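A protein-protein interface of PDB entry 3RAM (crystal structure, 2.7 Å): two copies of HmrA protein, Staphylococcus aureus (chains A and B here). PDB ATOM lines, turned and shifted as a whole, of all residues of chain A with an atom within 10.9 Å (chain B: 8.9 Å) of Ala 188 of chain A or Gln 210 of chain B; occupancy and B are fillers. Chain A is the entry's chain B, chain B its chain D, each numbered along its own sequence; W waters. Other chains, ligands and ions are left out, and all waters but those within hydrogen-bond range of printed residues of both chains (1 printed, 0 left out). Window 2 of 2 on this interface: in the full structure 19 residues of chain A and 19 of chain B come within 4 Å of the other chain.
O of Asp 196 of chain A sits close to OE1 of Gln 207 of chain B (3.3 Å). The side-chain amide nitrogen of Asn 193 of chain A sits at hydrogen-bond distance from a ring nitrogen (NE2) of His 211 of chain B. A ring nitrogen (NE2) of His 211 of chain B is in hydrogen-bond range of the side-chain carboxylate (OD1) of Asp 196 of chain A (3.4 Å). The backbone carbonyl oxygen (O) of Ala 188 of chain A is in hydrogen-bond range of a ring nitrogen (ND1) of His 211 of chain B (2.7 Å).
The side-chain hydroxyl of Ser 181 of chain A lies within hydrogen-bond range of the backbone carbonyl oxygen of Ile 232 of chain A, 2.8 Å away. The side-chain amide oxygen (OD1) of Asn 193 of chain A lies within hydrogen-bond range of the backbone NH (N) of Leu 195 of chain A, 2.9 Å away. The backbone carbonyl oxygen (O) of Ala 182 of chain A is in hydrogen-bond range of the backbone NH (N) of Ile 232 of chain A, at 2.8 Å. ND2 of Asn 193 of chain A is in hydrogen-bond range of OD1 of Asp 196 of chain A (3.1 Å). The backbone carbonyl oxygen (O) of His 183 of chain A lies within hydrogen-bond range of the backbone NH (N) of Ala 188 of chain A, 3.4 Å away.
Among the printed residues, pairs that only touch across the chains: Ala 188 of chain A with Gln 210 of chain B, Asp 189 of chain A with His 211 of chain B, Asp 189 of chain A with Lys 213 of chain B, Asn 193 of chain A with Gln 210 of chain B, Ile 199 of chain A with Gln 207 of chain B and Ile 232 of chain A with Gln 210 of chain B.
Of chain B, only Gln 210 and His 211 come within 4 Å of Ala 188 of chain A. Gln 210 of chain B touches three residues of chain A. No residue of chain B comes within 4 Å of Ala 191 of chain A. No residue of chain A comes within 4 Å of Ile 212 of chain B. Printed residues of chain B within 4 Å of Ile 199 of chain A: Gln 207. Printed residues of chain A within 4 Å of Lys 213 of chain B: Asp 189. Of the printed residues of chain A, Gln 207 of chain B touches Asp 196 and Ile 199. Printed residues of chain B within 4 Å of Asp 189 of chain A: His 211 and Lys 213. Printed residues of chain B within 4 Å of Ile 232 of chain A: Gln 210 (3.4 Å). The nearest residue of chain B that does not touch Ala 188 of chain A is Ile 212 of chain B (5.8 Å). The nearest residue of chain A that does not touch Gln 210 of chain B is Asp 196 of chain A (4.2 Å). The nearest printed residue of chain A that does not touch Gln 207 of chain B is Thr 268 of chain A (4.3 Å).
Among the printed residues, 10 pairs touch across the chains. Among the printed residues, no Asp or Glu carboxylate lies within 4 Å of a Lys or Arg side-chain nitrogen of the other chain.
No position is printed for both chains. Of the 10 pairs that touch across the chains among the printed residues, none has its exchanged pair printed and touching as well.
Water W1 lies within hydrogen-bond range of O of Ala 184 of chain A (2.7 Å) and OE1 of Gln 210 of chain B (2.8 Å).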
ATOM      1  N   GLY A 179      -9.820   5.362 -27.241  1.00  0.00           N
ATOM      2  CA  GLY A 179     -10.050   3.932 -27.004  1.00  0.00           C
ATOM      3  C   GLY A 179     -10.146   3.082 -28.260  1.00  0.00           C
ATOM      4  O   GLY A 179      -9.359   3.200 -29.181  1.00  0.00           O
ATOM      5  N   LYS A 180     -11.127   2.198 -28.281  1.00  0.00           N
ATOM      6  CA  LYS A 180     -11.267   1.208 -29.337  1.00  0.00           C
ATOM      7  C   LYS A 180     -12.775   0.976 -29.516  1.00  0.00           C
ATOM      8  O   LYS A 180     -13.473   0.615 -28.576  1.00  0.00           O
ATOM      9  CB  LYS A 180     -10.521  -0.077 -28.945  1.00  0.00           C
ATOM     10  CG  LYS A 180     -10.548  -1.168 -29.991  1.00  0.00           C
ATOM     11  CD  LYS A 180      -9.930  -2.451 -29.474  1.00  0.00           C
ATOM     12  CE  LYS A 180      -9.770  -3.460 -30.597  1.00  0.00           C
ATOM     13  NZ  LYS A 180      -9.883  -4.877 -30.119  1.00  0.00           N
ATOM     14  N   SER A 181     -13.278   1.240 -30.714  1.00  0.00           N
ATOM     15  CA  SER A 181     -14.699   1.148 -30.970  1.00  0.00           C
ATOM     16  C   SER A 181     -15.157  -0.281 -31.177  1.00  0.00           C
ATOM     17  O   SER A 181     -14.390  -1.164 -31.602  1.00  0.00           O
ATOM     18  CB  SER A 181     -15.071   1.976 -32.197  1.00  0.00           C
ATOM     19  OG  SER A 181     -15.159   3.349 -31.855  1.00  0.00           O
ATOM     20  N   ALA A 182     -16.435  -0.487 -30.888  1.00  0.00           N
ATOM     21  CA  ALA A 182     -17.085  -1.768 -31.085  1.00  0.00           C
ATOM     22  C   ALA A 182     -18.582  -1.540 -31.176  1.00  0.00           C
ATOM     23  O   ALA A 182     -19.084  -0.559 -30.672  1.00  0.00           O
ATOM     24  CB  ALA A 182     -16.752  -2.705 -29.937  1.00  0.00           C
ATOM     25  N   HIS A 183     -19.294  -2.442 -31.840  1.00  0.00           N
ATOM     26  CA  HIS A 183     -20.744  -2.379 -31.866  1.00  0.00           C
ATOM     27  C   HIS A 183     -21.179  -2.627 -30.421  1.00  0.00           C
ATOM     28  O   HIS A 183     -20.746  -3.598 -29.803  1.00  0.00           O
ATOM     29  CB  HIS A 183     -21.323  -3.410 -32.840  1.00  0.00           C
ATOM     30  CG  HIS A 183     -22.737  -3.128 -33.262  1.00  0.00           C
ATOM     31  ND1 HIS A 183     -23.837  -3.472 -32.494  1.00  0.00           N
ATOM     32  CD2 HIS A 183     -23.236  -2.553 -34.389  1.00  0.00           C
ATOM     33  CE1 HIS A 183     -24.946  -3.121 -33.128  1.00  0.00           C
ATOM     34  NE2 HIS A 183     -24.610  -2.562 -34.279  1.00  0.00           N
ATOM     35  N   ALA A 184     -22.000  -1.727 -29.887  1.00  0.00           N
ATOM     36  CA  ALA A 184     -22.317  -1.690 -28.462  1.00  0.00           C
ATOM     37  C   ALA A 184     -23.220  -2.836 -28.023  1.00  0.00           C
ATOM     38  O   ALA A 184     -23.181  -3.237 -26.861  1.00  0.00           O
ATOM     39  CB  ALA A 184     -22.961  -0.361 -28.110  1.00  0.00           C
ATOM     40  N   SER A 185     -24.036  -3.355 -28.941  1.00  0.00           N
ATOM     41  CA  SER A 185     -24.970  -4.432 -28.620  1.00  0.00           C
ATOM     42  C   SER A 185     -24.342  -5.791 -28.759  1.00  0.00           C
ATOM     43  O   SER A 185     -24.604  -6.677 -27.951  1.00  0.00           O
ATOM     44  CB  SER A 185     -26.196  -4.384 -29.521  1.00  0.00           C
ATOM     45  OG  SER A 185     -27.219  -3.615 -28.918  1.00  0.00           O
ATOM     46  N   GLU A 186     -23.532  -5.962 -29.798  1.00  0.00           N
ATOM     47  CA  GLU A 186     -23.015  -7.281 -30.167  1.00  0.00           C
ATOM     48  C   GLU A 186     -21.672  -7.606 -29.497  1.00  0.00           C
ATOM     49  O   GLU A 186     -21.511  -8.720 -28.983  1.00  0.00           O
ATOM     50  CB  GLU A 186     -22.868  -7.397 -31.690  1.00  0.00           C
ATOM     51  CG  GLU A 186     -24.094  -6.989 -32.530  1.00  0.00           C
ATOM     52  CD  GLU A 186     -23.762  -6.877 -34.046  1.00  0.00           C
ATOM     53  OE1 GLU A 186     -24.026  -5.807 -34.659  1.00  0.00           O
ATOM     54  OE2 GLU A 186     -23.222  -7.859 -34.624  1.00  0.00           O
ATOM     55  N   ASN A 187     -20.715  -6.669 -29.505  1.00  0.00           N
ATOM     56  CA  ASN A 187     -19.371  -6.967 -28.966  1.00  0.00           C
ATOM     57  C   ASN A 187     -18.665  -5.827 -28.223  1.00  0.00           C
ATOM     58  O   ASN A 187     -17.528  -5.465 -28.520  1.00  0.00           O
ATOM     59  CB  ASN A 187     -18.465  -7.585 -30.044  1.00  0.00           C
ATOM     60  CG  ASN A 187     -18.501  -6.826 -31.337  1.00  0.00           C
ATOM     61  OD1 ASN A 187     -18.006  -5.698 -31.425  1.00  0.00           O
ATOM     62  ND2 ASN A 187     -19.086  -7.443 -32.364  1.00  0.00           N
ATOM     63  N   ALA A 188     -19.354  -5.330 -27.199  1.00  0.00           N
ATOM     64  CA  ALA A 188     -18.862  -4.272 -26.343  1.00  0.00           C
ATOM     65  C   ALA A 188     -17.747  -4.758 -25.444  1.00  0.00           C
ATOM     66  O   ALA A 188     -17.055  -3.939 -24.854  1.00  0.00           O
ATOM     67  CB  ALA A 188     -20.006  -3.700 -25.492  1.00  0.00           C
ATOM     68  N   ASP A 189     -17.583  -6.073 -25.304  1.00  0.00           N
ATOM     69  CA  ASP A 189     -16.481  -6.606 -24.500  1.00  0.00           C
ATOM     70  C   ASP A 189     -15.109  -6.421 -25.198  1.00  0.00           C
ATOM     71  O   ASP A 189     -14.067  -6.526 -24.551  1.00  0.00           O
ATOM     72  CB  ASP A 189     -16.739  -8.061 -24.056  1.00  0.00           C
ATOM     73  CG  ASP A 189     -16.704  -9.070 -25.204  1.00  0.00           C
ATOM     74  OD1 ASP A 189     -17.152  -8.752 -26.335  1.00  0.00           O
ATOM     75  OD2 ASP A 189     -16.241 -10.208 -24.955  1.00  0.00           O
ATOM     76  N   GLU A 190     -15.110  -6.091 -26.493  1.00  0.00           N
ATOM     77  CA  GLU A 190     -13.866  -5.837 -27.224  1.00  0.00           C
ATOM     78  C   GLU A 190     -13.504  -4.347 -27.320  1.00  0.00           C
ATOM     79  O   GLU A 190     -12.540  -3.984 -28.013  1.00  0.00           O
ATOM     80  CB  GLU A 190     -13.973  -6.404 -28.635  1.00  0.00           C
ATOM     81  CG  GLU A 190     -14.118  -7.919 -28.707  1.00  0.00           C
ATOM     82  CD  GLU A 190     -14.431  -8.385 -30.119  1.00  0.00           C
ATOM     83  OE1 GLU A 190     -14.390  -7.535 -31.048  1.00  0.00           O
ATOM     84  OE2 GLU A 190     -14.724  -9.595 -30.295  1.00  0.00           O
ATOM     85  N   ALA A 191     -14.264  -3.499 -26.625  1.00  0.00           N
ATOM     86  CA  ALA A 191     -14.122  -2.058 -26.711  1.00  0.00           C
ATOM     87  C   ALA A 191     -13.274  -1.545 -25.580  1.00  0.00           C
ATOM     88  O   ALA A 191     -13.127  -2.197 -24.552  1.00  0.00           O
ATOM     89  CB  ALA A 191     -15.473  -1.403 -26.648  1.00  0.00           C
ATOM     90  N   LEU A 192     -12.709  -0.360 -25.799  1.00  0.00           N
ATOM     91  CA  LEU A 192     -12.111   0.474 -24.750  1.00  0.00           C
ATOM     92  C   LEU A 192     -12.869   1.792 -24.853  1.00  0.00           C
ATOM     93  O   LEU A 192     -12.763   2.489 -25.855  1.00  0.00           O
ATOM     94  CB  LEU A 192     -10.596   0.670 -24.970  1.00  0.00           C
ATOM     95  CG  LEU A 192      -9.721  -0.603 -24.895  1.00  0.00           C
ATOM     96  CD1 LEU A 192      -8.309  -0.333 -25.382  1.00  0.00           C
ATOM     97  CD2 LEU A 192      -9.706  -1.179 -23.486  1.00  0.00           C
ATOM     98  N   ASN A 193     -13.664   2.107 -23.836  1.00  0.00           N
ATOM     99  CA  ASN A 193     -14.704   3.132 -23.957  1.00  0.00           C
ATOM    100  C   ASN A 193     -14.212   4.545 -23.604  1.00  0.00           C
ATOM    101  O   ASN A 193     -14.060   4.890 -22.440  1.00  0.00           O
ATOM    102  CB  ASN A 193     -15.900   2.723 -23.087  1.00  0.00           C
ATOM    103  CG  ASN A 193     -17.141   3.548 -23.356  1.00  0.00           C
ATOM    104  OD1 ASN A 193     -17.063   4.637 -23.890  1.00  0.00           O
ATOM    105  ND2 ASN A 193     -18.291   3.033 -22.970  1.00  0.00           N
ATOM    106  N   ALA A 194     -13.986   5.367 -24.625  1.00  0.00           N
ATOM    107  CA  ALA A 194     -13.523   6.745 -24.425  1.00  0.00           C
ATOM    108  C   ALA A 194     -14.552   7.647 -23.770  1.00  0.00           C
ATOM    109  O   ALA A 194     -14.180   8.700 -23.237  1.00  0.00           O
ATOM    110  CB  ALA A 194     -13.088   7.363 -25.748  1.00  0.00           C
ATOM    111  N   LEU A 195     -15.836   7.278 -23.834  1.00  0.00           N
ATOM    112  CA  LEU A 195     -16.884   8.075 -23.185  1.00  0.00           C
ATOM    113  C   LEU A 195     -16.958   7.747 -21.705  1.00  0.00           C
ATOM    114  O   LEU A 195     -17.208   8.635 -20.900  1.00  0.00           O
ATOM    115  CB  LEU A 195     -18.254   7.866 -23.843  1.00  0.00           C
ATOM    116  CG  LEU A 195     -19.446   8.765 -23.426  1.00  0.00           C
ATOM    117  CD1 LEU A 195     -19.053  10.226 -23.296  1.00  0.00           C
ATOM    118  CD2 LEU A 195     -20.602   8.618 -24.411  1.00  0.00           C
ATOM    119  N   ASP A 196     -16.747   6.482 -21.343  1.00  0.00           N
ATOM    120  CA  ASP A 196     -16.671   6.104 -19.928  1.00  0.00           C
ATOM    121  C   ASP A 196     -15.494   6.816 -19.302  1.00  0.00           C
ATOM    122  O   ASP A 196     -15.598   7.261 -18.159  1.00  0.00           O
ATOM    123  CB  ASP A 196     -16.543   4.583 -19.715  1.00  0.00           C
ATOM    124  CG  ASP A 196     -17.886   3.853 -19.827  1.00  0.00           C
ATOM    125  OD1 ASP A 196     -17.894   2.581 -19.909  1.00  0.00           O
ATOM    126  OD2 ASP A 196     -18.935   4.570 -19.824  1.00  0.00           O
ATOM    127  N   ALA A 197     -14.390   6.942 -20.045  1.00  0.00           N
ATOM    128  CA  ALA A 197     -13.228   7.708 -19.576  1.00  0.00           C
ATOM    129  C   ALA A 197     -13.625   9.161 -19.263  1.00  0.00           C
ATOM    130  O   ALA A 197     -13.304   9.684 -18.195  1.00  0.00           O
ATOM    131  CB  ALA A 197     -12.089   7.656 -20.597  1.00  0.00           C
ATOM    132  N   ILE A 199     -16.711  10.506 -18.699  1.00  0.00           N
ATOM    133  CA  ILE A 199     -17.645  10.565 -17.570  1.00  0.00           C
ATOM    134  C   ILE A 199     -16.872  10.453 -16.243  1.00  0.00           C
ATOM    135  O   ILE A 199     -17.124  11.197 -15.295  1.00  0.00           O
ATOM    136  CB  ILE A 199     -18.705   9.421 -17.652  1.00  0.00           C
ATOM    137  CG1 ILE A 199     -19.569   9.555 -18.920  1.00  0.00           C
ATOM    138  CG2 ILE A 199     -19.573   9.383 -16.400  1.00  0.00           C
ATOM    139  CD1 ILE A 199     -20.340  10.820 -19.016  1.00  0.00           C
ATOM    140  N   ALA A 228     -22.315   7.869 -32.837  1.00  0.00           N
ATOM    141  CA  ALA A 228     -23.305   6.825 -33.146  1.00  0.00           C
ATOM    142  C   ALA A 228     -23.668   6.050 -31.882  1.00  0.00           C
ATOM    143  O   ALA A 228     -22.797   5.500 -31.212  1.00  0.00           O
ATOM    144  CB  ALA A 228     -22.784   5.890 -34.215  1.00  0.00           C
ATOM    145  N   ALA A 229     -24.964   6.018 -31.573  1.00  0.00           N
ATOM    146  CA  ALA A 229     -25.463   5.425 -30.334  1.00  0.00           C
ATOM    147  C   ALA A 229     -25.178   3.923 -30.259  1.00  0.00           C
ATOM    148  O   ALA A 229     -24.943   3.378 -29.161  1.00  0.00           O
ATOM    149  CB  ALA A 229     -26.954   5.693 -30.189  1.00  0.00           C
ATOM    150  N   ASN A 230     -25.178   3.270 -31.426  1.00  0.00           N
ATOM    151  CA  ASN A 230     -24.908   1.826 -31.534  1.00  0.00           C
ATOM    152  C   ASN A 230     -23.426   1.395 -31.454  1.00  0.00           C
ATOM    153  O   ASN A 230     -23.146   0.202 -31.430  1.00  0.00           O
ATOM    154  CB  ASN A 230     -25.545   1.258 -32.817  1.00  0.00           C
ATOM    155  CG  ASN A 230     -25.100   1.997 -34.099  1.00  0.00           C
ATOM    156  OD1 ASN A 230     -24.886   3.216 -34.105  1.00  0.00           O
ATOM    157  ND2 ASN A 230     -24.989   1.251 -35.193  1.00  0.00           N
ATOM    158  N   ILE A 231     -22.505   2.359 -31.409  1.00  0.00           N
ATOM    159  CA  ILE A 231     -21.065   2.118 -31.436  1.00  0.00           C
ATOM    160  C   ILE A 231     -20.417   2.760 -30.230  1.00  0.00           C
ATOM    161  O   ILE A 231     -20.671   3.928 -29.942  1.00  0.00           O
ATOM    162  CB  ILE A 231     -20.412   2.774 -32.659  1.00  0.00           C
ATOM    163  CG1 ILE A 231     -20.952   2.179 -33.945  1.00  0.00           C
ATOM    164  CG2 ILE A 231     -18.911   2.575 -32.638  1.00  0.00           C
ATOM    165  CD1 ILE A 231     -20.411   2.879 -35.172  1.00  0.00           C
ATOM    166  N   ILE A 232     -19.566   2.007 -29.537  1.00  0.00           N
ATOM    167  CA  ILE A 232     -18.827   2.518 -28.381  1.00  0.00           C
ATOM    168  C   ILE A 232     -17.772   3.546 -28.850  1.00  0.00           C
ATOM    169  O   ILE A 232     -17.007   3.267 -29.778  1.00  0.00           O
ATOM    170  CB  ILE A 232     -18.142   1.372 -27.614  1.00  0.00           C
ATOM    171  CG1 ILE A 232     -19.187   0.406 -27.024  1.00  0.00           C
ATOM    172  CG2 ILE A 232     -17.210   1.910 -26.548  1.00  0.00           C
ATOM    173  CD1 ILE A 232     -20.240   1.051 -26.143  1.00  0.00           C
ATOM    174  N   PRO A 233     -17.747   4.750 -28.237  1.00  0.00           N
ATOM    175  CA  PRO A 233     -16.804   5.780 -28.688  1.00  0.00           C
ATOM    176  C   PRO A 233     -15.320   5.464 -28.468  1.00  0.00           C
ATOM    177  O   PRO A 233     -14.923   5.045 -27.379  1.00  0.00           O
ATOM    178  CB  PRO A 233     -17.222   7.015 -27.861  1.00  0.00           C
ATOM    179  CG  PRO A 233     -18.629   6.774 -27.510  1.00  0.00           C
ATOM    180  CD  PRO A 233     -18.689   5.305 -27.245  1.00  0.00           C
ATOM    181  N   THR A 268     -10.376   2.882 -17.469  1.00  0.00           N
ATOM    182  CA  THR A 268     -11.127   2.440 -18.657  1.00  0.00           C
ATOM    183  C   THR A 268     -10.284   1.737 -19.733  1.00  0.00           C
ATOM    184  O   THR A 268     -10.832   1.307 -20.757  1.00  0.00           O
ATOM    185  CB  THR A 268     -11.822   3.636 -19.348  1.00  0.00           C
ATOM    186  OG1 THR A 268     -10.824   4.505 -19.900  1.00  0.00           O
ATOM    187  CG2 THR A 268     -12.712   4.420 -18.366  1.00  0.00           C
ATOM    188  N   GLY B 204     -16.620   3.370 -11.452  1.00  0.00           N
ATOM    189  CA  GLY B 204     -15.815   2.675 -12.457  1.00  0.00           C
ATOM    190  C   GLY B 204     -16.244   1.229 -12.652  1.00  0.00           C
ATOM    191  O   GLY B 204     -16.354   0.755 -13.792  1.00  0.00           O
ATOM    192  N   VAL B 205     -16.499   0.525 -11.547  1.00  0.00           N
ATOM    193  CA  VAL B 205     -17.041  -0.831 -11.625  1.00  0.00           C
ATOM    194  C   VAL B 205     -18.392  -0.851 -12.366  1.00  0.00           C
ATOM    195  O   VAL B 205     -18.655  -1.770 -13.140  1.00  0.00           O
ATOM    196  CB  VAL B 205     -17.185  -1.483 -10.216  1.00  0.00           C
ATOM    197  CG1 VAL B 205     -17.909  -2.834 -10.299  1.00  0.00           C
ATOM    198  CG2 VAL B 205     -15.813  -1.636  -9.556  1.00  0.00           C
ATOM    199  N   ALA B 206     -19.234   0.159 -12.134  1.00  0.00           N
ATOM    200  CA  ALA B 206     -20.544   0.234 -12.782  1.00  0.00           C
ATOM    201  C   ALA B 206     -20.398   0.271 -14.305  1.00  0.00           C
ATOM    202  O   ALA B 206     -21.126  -0.409 -15.040  1.00  0.00           O
ATOM    203  CB  ALA B 206     -21.314   1.440 -12.288  1.00  0.00           C
ATOM    204  N   GLN B 207     -19.430   1.063 -14.749  1.00  0.00           N
ATOM    205  CA  GLN B 207     -19.112   1.249 -16.162  1.00  0.00           C
ATOM    206  C   GLN B 207     -18.545  -0.012 -16.809  1.00  0.00           C
ATOM    207  O   GLN B 207     -18.842  -0.281 -17.973  1.00  0.00           O
ATOM    208  CB  GLN B 207     -18.109   2.409 -16.329  1.00  0.00           C
ATOM    209  CG  GLN B 207     -18.722   3.811 -16.146  1.00  0.00           C
ATOM    210  CD  GLN B 207     -17.697   4.950 -16.166  1.00  0.00           C
ATOM    211  OE1 GLN B 207     -16.471   4.739 -16.222  1.00  0.00           O
ATOM    212  NE2 GLN B 207     -18.207   6.174 -16.109  1.00  0.00           N
ATOM    213  N   LEU B 208     -17.739  -0.761 -16.051  1.00  0.00           N
ATOM    214  CA  LEU B 208     -17.115  -2.023 -16.498  1.00  0.00           C
ATOM    215  C   LEU B 208     -18.121  -3.083 -16.943  1.00  0.00           C
ATOM    216  O   LEU B 208     -17.820  -3.917 -17.816  1.00  0.00           O
ATOM    217  CB  LEU B 208     -16.246  -2.613 -15.374  1.00  0.00           C
ATOM    218  CG  LEU B 208     -15.560  -3.972 -15.572  1.00  0.00           C
ATOM    219  CD1 LEU B 208     -14.711  -3.983 -16.843  1.00  0.00           C
ATOM    220  CD2 LEU B 208     -14.734  -4.343 -14.334  1.00  0.00           C
ATOM    221  N   ARG B 209     -19.302  -3.068 -16.333  1.00  0.00           N
ATOM    222  CA  ARG B 209     -20.296  -4.100 -16.586  1.00  0.00           C
ATOM    223  C   ARG B 209     -20.799  -4.116 -18.008  1.00  0.00           C
ATOM    224  O   ARG B 209     -21.227  -5.155 -18.494  1.00  0.00           O
ATOM    225  CB  ARG B 209     -21.481  -3.919 -15.666  1.00  0.00           C
ATOM    226  CG  ARG B 209     -21.212  -4.195 -14.206  1.00  0.00           C
ATOM    227  CD  ARG B 209     -22.398  -3.626 -13.409  1.00  0.00           C
ATOM    228  NE  ARG B 209     -22.051  -3.366 -12.023  1.00  0.00           N
ATOM    229  CZ  ARG B 209     -21.803  -4.326 -11.158  1.00  0.00           C
ATOM    230  NH1 ARG B 209     -21.889  -5.591 -11.558  1.00  0.00           N
ATOM    231  NH2 ARG B 209     -21.468  -4.024  -9.903  1.00  0.00           N
ATOM    232  N   GLN B 210     -20.760  -2.970 -18.677  1.00  0.00           N
ATOM    233  CA  GLN B 210     -21.061  -2.931 -20.117  1.00  0.00           C
ATOM    234  C   GLN B 210     -20.086  -3.801 -20.940  1.00  0.00           C
ATOM    235  O   GLN B 210     -20.459  -4.370 -21.976  1.00  0.00           O
ATOM    236  CB  GLN B 210     -21.069  -1.496 -20.655  1.00  0.00           C
ATOM    237  CG  GLN B 210     -21.629  -1.432 -22.061  1.00  0.00           C
ATOM    238  CD  GLN B 210     -21.780  -0.047 -22.626  1.00  0.00           C
ATOM    239  OE1 GLN B 210     -22.397   0.118 -23.671  1.00  0.00           O
ATOM    240  NE2 GLN B 210     -21.214   0.956 -21.954  1.00  0.00           N
ATOM    241  N   HIS B 211     -18.858  -3.929 -20.437  1.00  0.00           N
ATOM    242  CA  HIS B 211     -17.753  -4.489 -21.199  1.00  0.00           C
ATOM    243  C   HIS B 211     -17.234  -5.843 -20.691  1.00  0.00           C
ATOM    244  O   HIS B 211     -16.199  -6.315 -21.151  1.00  0.00           O
ATOM    245  CB  HIS B 211     -16.624  -3.458 -21.241  1.00  0.00           C
ATOM    246  CG  HIS B 211     -17.067  -2.121 -21.749  1.00  0.00           C
ATOM    247  ND1 HIS B 211     -17.306  -1.874 -23.081  1.00  0.00           N
ATOM    248  CD2 HIS B 211     -17.337  -0.966 -21.099  1.00  0.00           C
ATOM    249  CE1 HIS B 211     -17.708  -0.625 -23.228  1.00  0.00           C
ATOM    250  NE2 HIS B 211     -17.735  -0.052 -22.041  1.00  0.00           N
ATOM    251  N   ILE B 212     -17.943  -6.490 -19.776  1.00  0.00           N
ATOM    252  CA  ILE B 212     -17.564  -7.842 -19.381  1.00  0.00           C
ATOM    253  C   ILE B 212     -18.475  -8.879 -20.053  1.00  0.00           C
ATOM    254  O   ILE B 212     -19.610  -8.578 -20.430  1.00  0.00           O
ATOM    255  CB  ILE B 212     -17.488  -8.011 -17.838  1.00  0.00           C
ATOM    256  CG1 ILE B 212     -18.874  -7.949 -17.178  1.00  0.00           C
ATOM    257  CG2 ILE B 212     -16.517  -6.987 -17.256  1.00  0.00           C
ATOM    258  CD1 ILE B 212     -18.828  -8.016 -15.658  1.00  0.00           C
ATOM    259  N   LYS B 213     -17.956 -10.096 -20.228  1.00  0.00           N
ATOM    260  CA  LYS B 213     -18.691 -11.139 -20.943  1.00  0.00           C
ATOM    261  C   LYS B 213     -19.964 -11.436 -20.181  1.00  0.00           C
ATOM    262  O   LYS B 213     -20.037 -11.172 -18.989  1.00  0.00           O
ATOM    263  CB  LYS B 213     -17.855 -12.412 -21.103  1.00  0.00           C
ATOM    264  CG  LYS B 213     -16.570 -12.248 -21.920  1.00  0.00           C
ATOM    265  CD  LYS B 213     -16.018 -13.601 -22.337  1.00  0.00           C
ATOM    266  CE  LYS B 213     -14.727 -13.483 -23.148  1.00  0.00           C
ATOM    267  NZ  LYS B 213     -14.522 -14.690 -24.051  1.00  0.00           N
ATOM    268  N   LYS B 214     -20.972 -11.981 -20.858  1.00  0.00           N
ATOM    269  CA  LYS B 214     -22.295 -12.139 -20.229  1.00  0.00           C
ATOM    270  C   LYS B 214     -22.319 -13.199 -19.123  1.00  0.00           C
ATOM    271  O   LYS B 214     -23.278 -13.249 -18.348  1.00  0.00           O
ATOM    272  CB  LYS B 214     -23.404 -12.383 -21.283  1.00  0.00           C
ATOM    273  CG  LYS B 214     -23.842 -11.087 -22.064  1.00  0.00           C
ATOM    274  CD  LYS B 214     -24.560 -10.012 -21.165  1.00  0.00           C
ATOM    275  CE  LYS B 214     -24.019  -8.545 -21.353  1.00  0.00           C
ATOM    276  NZ  LYS B 214     -22.860  -8.151 -20.424  1.00  0.00           N
ATOM    277  N   VAL B 218     -19.306  -9.045 -11.235  1.00  0.00           N
ATOM    278  CA  VAL B 218     -18.517  -8.277 -10.266  1.00  0.00           C
ATOM    279  C   VAL B 218     -19.542  -7.600  -9.370  1.00  0.00           C
ATOM    280  O   VAL B 218     -20.477  -7.007  -9.869  1.00  0.00           O
ATOM    281  CB  VAL B 218     -17.576  -7.261 -10.979  1.00  0.00           C
ATOM    282  CG1 VAL B 218     -18.340  -6.474 -12.006  1.00  0.00           C
ATOM    283  CG2 VAL B 218     -16.869  -6.349  -9.987  1.00  0.00           C
ATOM    284  N   LYS B 256      -8.735  -6.149 -14.355  1.00  0.00           N
ATOM    285  CA  LYS B 256      -9.467  -4.961 -14.801  1.00  0.00           C
ATOM    286  C   LYS B 256     -10.013  -4.202 -13.609  1.00  0.00           C
ATOM    287  O   LYS B 256      -9.904  -2.980 -13.546  1.00  0.00           O
ATOM    288  CB  LYS B 256     -10.608  -5.318 -15.748  1.00  0.00           C
ATOM    289  CG  LYS B 256     -10.145  -5.678 -17.150  1.00  0.00           C
ATOM    290  CD  LYS B 256     -11.320  -6.083 -18.020  1.00  0.00           C
ATOM    291  CE  LYS B 256     -10.914  -6.499 -19.444  1.00  0.00           C
ATOM    292  NZ  LYS B 256     -12.016  -7.301 -20.106  1.00  0.00           N
HETATM  293  O   HOH W   1     -23.983  -2.017 -24.624  1.00  0.00           O
